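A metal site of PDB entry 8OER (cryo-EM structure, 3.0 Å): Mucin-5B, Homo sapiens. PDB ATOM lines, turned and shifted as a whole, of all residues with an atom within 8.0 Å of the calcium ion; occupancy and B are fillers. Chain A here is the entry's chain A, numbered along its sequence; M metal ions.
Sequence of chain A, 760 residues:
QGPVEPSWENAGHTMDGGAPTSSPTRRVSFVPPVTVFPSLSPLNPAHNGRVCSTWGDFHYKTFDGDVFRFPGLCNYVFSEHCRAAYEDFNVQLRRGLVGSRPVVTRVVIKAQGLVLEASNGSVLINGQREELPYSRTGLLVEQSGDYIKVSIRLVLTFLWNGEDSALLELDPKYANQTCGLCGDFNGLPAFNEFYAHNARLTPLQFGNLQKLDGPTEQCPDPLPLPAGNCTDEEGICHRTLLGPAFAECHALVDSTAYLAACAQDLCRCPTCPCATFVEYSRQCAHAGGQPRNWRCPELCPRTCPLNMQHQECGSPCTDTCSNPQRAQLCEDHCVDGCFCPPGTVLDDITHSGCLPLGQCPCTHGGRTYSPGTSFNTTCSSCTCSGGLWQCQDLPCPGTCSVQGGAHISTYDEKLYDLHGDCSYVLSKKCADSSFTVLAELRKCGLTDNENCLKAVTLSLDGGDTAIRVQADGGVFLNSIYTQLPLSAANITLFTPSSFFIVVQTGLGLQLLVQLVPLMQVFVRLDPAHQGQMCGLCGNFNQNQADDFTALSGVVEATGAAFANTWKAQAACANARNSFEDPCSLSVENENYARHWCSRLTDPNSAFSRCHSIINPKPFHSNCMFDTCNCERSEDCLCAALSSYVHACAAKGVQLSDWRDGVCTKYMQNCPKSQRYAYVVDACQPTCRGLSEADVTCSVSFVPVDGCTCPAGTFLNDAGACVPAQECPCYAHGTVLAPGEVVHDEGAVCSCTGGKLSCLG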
ATOM      1  N   THR A  62      13.069  24.969 -25.746  1.00  0.00           N
ATOM      2  CA  THR A  62      14.211  25.017 -24.859  1.00  0.00           C
ATOM      3  C   THR A  62      14.845  26.399 -24.883  1.00  0.00           C
ATOM      4  O   THR A  62      14.429  27.295 -25.618  1.00  0.00           O
ATOM      5  CB  THR A  62      15.241  23.958 -25.249  1.00  0.00           C
ATOM      6  OG1 THR A  62      16.151  24.510 -26.215  1.00  0.00           O
ATOM      7  CG2 THR A  62      14.568  22.726 -25.820  1.00  0.00           C
ATOM      8  N   PHE A  63      15.887  26.580 -24.067  1.00  0.00           N
ATOM      9  CA  PHE A  63      16.517  27.891 -23.944  1.00  0.00           C
ATOM     10  C   PHE A  63      17.092  28.352 -25.273  1.00  0.00           C
ATOM     11  O   PHE A  63      16.962  29.533 -25.635  1.00  0.00           O
ATOM     12  CB  PHE A  63      17.630  27.848 -22.901  1.00  0.00           C
ATOM     13  CG  PHE A  63      17.144  27.576 -21.517  1.00  0.00           C
ATOM     14  CD1 PHE A  63      16.023  28.206 -21.025  1.00  0.00           C
ATOM     15  CD2 PHE A  63      17.841  26.713 -20.700  1.00  0.00           C
ATOM     16  CE1 PHE A  63      15.593  27.960 -19.745  1.00  0.00           C
ATOM     17  CE2 PHE A  63      17.424  26.461 -19.423  1.00  0.00           C
ATOM     18  CZ  PHE A  63      16.288  27.085 -18.947  1.00  0.00           C
ATOM     19  N   ASP A  64      17.732  27.460 -26.010  1.00  0.00           N
ATOM     20  CA  ASP A  64      18.578  27.838 -27.136  1.00  0.00           C
ATOM     21  C   ASP A  64      17.807  27.946 -28.445  1.00  0.00           C
ATOM     22  O   ASP A  64      18.405  28.276 -29.470  1.00  0.00           O
ATOM     23  CB  ASP A  64      19.729  26.848 -27.265  1.00  0.00           C
ATOM     24  CG  ASP A  64      20.036  26.153 -25.967  1.00  0.00           C
ATOM     25  OD1 ASP A  64      20.015  26.829 -24.911  1.00  0.00           O
ATOM     26  OD2 ASP A  64      20.304  24.934 -25.987  1.00  0.00           O
ATOM     27  N   ASP A  66      15.209  25.505 -29.612  1.00  0.00           N
ATOM     28  CA  ASP A  66      14.564  24.316 -30.123  1.00  0.00           C
ATOM     29  C   ASP A  66      13.074  24.312 -29.801  1.00  0.00           C
ATOM     30  O   ASP A  66      12.624  24.947 -28.845  1.00  0.00           O
ATOM     31  CB  ASP A  66      15.216  23.062 -29.559  1.00  0.00           C
ATOM     32  CG  ASP A  66      16.617  22.894 -30.054  1.00  0.00           C
ATOM     33  OD1 ASP A  66      17.121  23.826 -30.708  1.00  0.00           O
ATOM     34  OD2 ASP A  66      17.223  21.849 -29.786  1.00  0.00           O
ATOM     35  N   ASN A 176      24.803  26.118 -18.807  1.00  0.00           N
ATOM     36  CA  ASN A 176      25.565  24.873 -18.895  1.00  0.00           C
ATOM     37  C   ASN A 176      25.439  24.010 -17.637  1.00  0.00           C
ATOM     38  O   ASN A 176      25.954  22.897 -17.607  1.00  0.00           O
ATOM     39  CB  ASN A 176      27.035  25.156 -19.174  1.00  0.00           C
ATOM     40  CG  ASN A 176      27.651  24.155 -20.121  1.00  0.00           C
ATOM     41  OD1 ASN A 176      27.029  23.157 -20.475  1.00  0.00           O
ATOM     42  ND2 ASN A 176      28.885  24.419 -20.527  1.00  0.00           N
ATOM     43  N   CYS A 182      13.876  21.898 -20.642  1.00  0.00           N
ATOM     44  CA  CYS A 182      14.304  23.221 -21.081  1.00  0.00           C
ATOM     45  C   CYS A 182      15.712  23.222 -21.652  1.00  0.00           C
ATOM     46  O   CYS A 182      16.140  24.258 -22.170  1.00  0.00           O
ATOM     47  CB  CYS A 182      14.205  24.232 -19.930  1.00  0.00           C
ATOM     48  SG  CYS A 182      12.523  24.643 -19.414  1.00  0.00           S
ATOM     49  N   GLY A 183      16.440  22.129 -21.561  1.00  0.00           N
ATOM     50  CA  GLY A 183      17.722  22.043 -22.231  1.00  0.00           C
ATOM     51  C   GLY A 183      18.910  22.223 -21.311  1.00  0.00           C
ATOM     52  O   GLY A 183      18.799  21.965 -20.112  1.00  0.00           O
ATOM     53  N   ASP A 184      20.039  22.670 -21.856  1.00  0.00           N
ATOM     54  CA  ASP A 184      21.234  22.849 -21.044  1.00  0.00           C
ATOM     55  C   ASP A 184      21.677  24.288 -20.892  1.00  0.00           C
ATOM     56  O   ASP A 184      22.595  24.542 -20.113  1.00  0.00           O
ATOM     57  CB  ASP A 184      22.412  22.056 -21.626  1.00  0.00           C
ATOM     58  CG  ASP A 184      22.575  22.271 -23.107  1.00  0.00           C
ATOM     59  OD1 ASP A 184      22.097  23.311 -23.591  1.00  0.00           O
ATOM     60  OD2 ASP A 184      23.203  21.418 -23.773  1.00  0.00           O
ATOM     61  N   PHE A 185      21.089  25.242 -21.627  1.00  0.00           N
ATOM     62  CA  PHE A 185      21.433  26.658 -21.496  1.00  0.00           C
ATOM     63  C   PHE A 185      22.887  26.934 -21.863  1.00  0.00           C
ATOM     64  O   PHE A 185      23.509  27.863 -21.344  1.00  0.00           O
ATOM     65  CB  PHE A 185      21.118  27.171 -20.093  1.00  0.00           C
ATOM     66  CG  PHE A 185      20.943  28.655 -19.997  1.00  0.00           C
ATOM     67  CD1 PHE A 185      20.872  29.445 -21.125  1.00  0.00           C
ATOM     68  CD2 PHE A 185      20.838  29.266 -18.762  1.00  0.00           C
ATOM     69  CE1 PHE A 185      20.718  30.798 -21.029  1.00  0.00           C
ATOM     70  CE2 PHE A 185      20.683  30.630 -18.656  1.00  0.00           C
ATOM     71  CZ  PHE A 185      20.615  31.399 -19.793  1.00  0.00           C
ATOM     72  N   ASN A 186      23.441  26.124 -22.775  1.00  0.00           N
ATOM     73  CA  ASN A 186      24.778  26.367 -23.292  1.00  0.00           C
ATOM     74  C   ASN A 186      24.771  27.270 -24.516  1.00  0.00           C
ATOM     75  O   ASN A 186      25.842  27.646 -25.004  1.00  0.00           O
ATOM     76  CB  ASN A 186      25.465  25.047 -23.643  1.00  0.00           C
ATOM     77  CG  ASN A 186      24.710  24.260 -24.687  1.00  0.00           C
ATOM     78  OD1 ASN A 186      23.694  24.707 -25.211  1.00  0.00           O
ATOM     79  ND2 ASN A 186      25.204  23.066 -24.997  1.00  0.00           N
ATOM     80  N   GLY A 187      23.593  27.611 -25.032  1.00  0.00           N
ATOM     81  CA  GLY A 187      23.458  28.484 -26.172  1.00  0.00           C
ATOM     82  C   GLY A 187      23.424  27.813 -27.517  1.00  0.00           C
ATOM     83  O   GLY A 187      23.057  28.465 -28.509  1.00  0.00           O
ATOM     84  N   LEU A 188      23.761  26.532 -27.591  1.00  0.00           N
ATOM     85  CA  LEU A 188      23.788  25.820 -28.864  1.00  0.00           C
ATOM     86  C   LEU A 188      22.522  24.993 -28.997  1.00  0.00           C
ATOM     87  O   LEU A 188      22.378  23.961 -28.321  1.00  0.00           O
ATOM     88  CB  LEU A 188      25.020  24.922 -28.955  1.00  0.00           C
ATOM     89  CG  LEU A 188      26.340  25.701 -28.937  1.00  0.00           C
ATOM     90  CD1 LEU A 188      27.509  24.769 -28.722  1.00  0.00           C
ATOM     91  CD2 LEU A 188      26.508  26.460 -30.236  1.00  0.00           C
ATOM     92  N   PRO A 189      21.590  25.385 -29.854  1.00  0.00           N
ATOM     93  CA  PRO A 189      20.280  24.736 -29.881  1.00  0.00           C
ATOM     94  C   PRO A 189      20.309  23.317 -30.415  1.00  0.00           C
ATOM     95  O   PRO A 189      19.879  22.380 -29.741  1.00  0.00           O
ATOM     96  CB  PRO A 189      19.449  25.635 -30.800  1.00  0.00           C
ATOM     97  CG  PRO A 189      20.397  26.481 -31.530  1.00  0.00           C
ATOM     98  CD  PRO A 189      21.690  26.511 -30.801  1.00  0.00           C
ATOM     99  N   ALA A 190      20.834  23.144 -31.618  1.00  0.00           N
ATOM    100  CA  ALA A 190      20.554  21.963 -32.416  1.00  0.00           C
ATOM    101  C   ALA A 190      21.518  20.816 -32.167  1.00  0.00           C
ATOM    102  O   ALA A 190      21.432  19.808 -32.876  1.00  0.00           O
ATOM    103  CB  ALA A 190      20.567  22.327 -33.904  1.00  0.00           C
ATOM    104  N   PHE A 191      22.438  20.917 -31.201  1.00  0.00           N
ATOM    105  CA  PHE A 191      23.540  19.966 -31.237  1.00  0.00           C
ATOM    106  C   PHE A 191      23.723  19.263 -29.890  1.00  0.00           C
ATOM    107  O   PHE A 191      24.233  18.137 -29.857  1.00  0.00           O
ATOM    108  CB  PHE A 191      24.822  20.720 -31.687  1.00  0.00           C
ATOM    109  CG  PHE A 191      26.124  20.146 -31.189  1.00  0.00           C
ATOM    110  CD1 PHE A 191      27.114  20.995 -30.736  1.00  0.00           C
ATOM    111  CD2 PHE A 191      26.434  18.810 -31.364  1.00  0.00           C
ATOM    112  CE1 PHE A 191      28.329  20.495 -30.327  1.00  0.00           C
ATOM    113  CE2 PHE A 191      27.637  18.296 -30.939  1.00  0.00           C
ATOM    114  CZ  PHE A 191      28.589  19.145 -30.433  1.00  0.00           C
ATOM    115  N   ASN A 192      23.253  19.842 -28.786  1.00  0.00           N
ATOM    116  CA  ASN A 192      23.659  19.242 -27.528  1.00  0.00           C
ATOM    117  C   ASN A 192      22.522  18.793 -26.613  1.00  0.00           C
ATOM    118  O   ASN A 192      22.773  18.188 -25.561  1.00  0.00           O
ATOM    119  CB  ASN A 192      24.559  20.207 -26.769  1.00  0.00           C
ATOM    120  CG  ASN A 192      25.406  19.506 -25.744  1.00  0.00           C
ATOM    121  OD1 ASN A 192      25.761  18.344 -25.912  1.00  0.00           O
ATOM    122  ND2 ASN A 192      25.728  20.202 -24.666  1.00  0.00           N
ATOM    123  N   GLU A 193      21.269  19.027 -26.999  1.00  0.00           N
ATOM    124  CA  GLU A 193      20.170  18.567 -26.146  1.00  0.00           C
ATOM    125  C   GLU A 193      19.858  17.096 -26.363  1.00  0.00           C
ATOM    126  O   GLU A 193      19.392  16.428 -25.439  1.00  0.00           O
ATOM    127  CB  GLU A 193      18.895  19.368 -26.407  1.00  0.00           C
ATOM    128  CG  GLU A 193      18.964  20.864 -26.164  1.00  0.00           C
ATOM    129  CD  GLU A 193      20.029  21.278 -25.185  1.00  0.00           C
ATOM    130  OE1 GLU A 193      20.873  22.120 -25.570  1.00  0.00           O
ATOM    131  OE2 GLU A 193      20.016  20.810 -24.030  1.00  0.00           O
ATOM    132  N   PHE A 194      20.118  16.581 -27.571  1.00  0.00           N
ATOM    133  CA  PHE A 194      19.648  15.273 -28.004  1.00  0.00           C
ATOM    134  C   PHE A 194      20.800  14.361 -28.385  1.00  0.00           C
ATOM    135  O   PHE A 194      20.778  13.744 -29.446  1.00  0.00           O
ATOM    136  CB  PHE A 194      18.675  15.401 -29.173  1.00  0.00           C
ATOM    137  CG  PHE A 194      17.894  16.669 -29.155  1.00  0.00           C
ATOM    138  CD1 PHE A 194      18.388  17.799 -29.778  1.00  0.00           C
ATOM    139  CD2 PHE A 194      16.676  16.733 -28.511  1.00  0.00           C
ATOM    140  CE1 PHE A 194      17.672  18.962 -29.766  1.00  0.00           C
ATOM    141  CE2 PHE A 194      15.959  17.897 -28.499  1.00  0.00           C
ATOM    142  CZ  PHE A 194      16.457  19.017 -29.122  1.00  0.00           C
HETATM  143 CA    CA M   1      22.751  22.917 -26.306  1.00  0.00          CA
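The side-chain carboxylate of Asp 64 sits close to the side-chain amide oxygen of Asn 186 (3.5 Å). OD2 of Asp 184 sits at hydrogen-bond distance from ND2 of Asn 192, 2.9 Å away. O of Asp 184 is in hydrogen-bond range of N of Asn 176 (3.0 Å). ND2 of Asn 186 lies close to ND2 of Asn 192. The backbone NH of Asp 64 lies close to the side-chain hydroxyl of Thr 62.
OD2 of Asp 64 touches the calcium ion, at 3.2 Å. Asn 192 touches the calcium ion. Of the 18 residues printed, 6 come within 4 Å of the calcium ion. The nearest printed residue that does not touch the calcium ion is Pro 189 (4.5 Å).
The calcium ion is bound by OE1 of Glu 193 (2.2 Å). The calcium ion is bound by the side-chain amide oxygen (OD1) of Asn 186, at 2.3 Å. The calcium ion is bound by O of Leu 188 (2.3 Å). The side-chain amide nitrogen (ND2) of Asn 186 is bound to the calcium ion, 2.8 Å away. The calcium ion is bound by the side-chain carboxylate (OD1) of Asp 184 (2.8 Å). The calcium ion has five donor atoms within binding distance. Slightly farther from the calcium ion lies OD2 of Asp 184 (3.0 Å).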
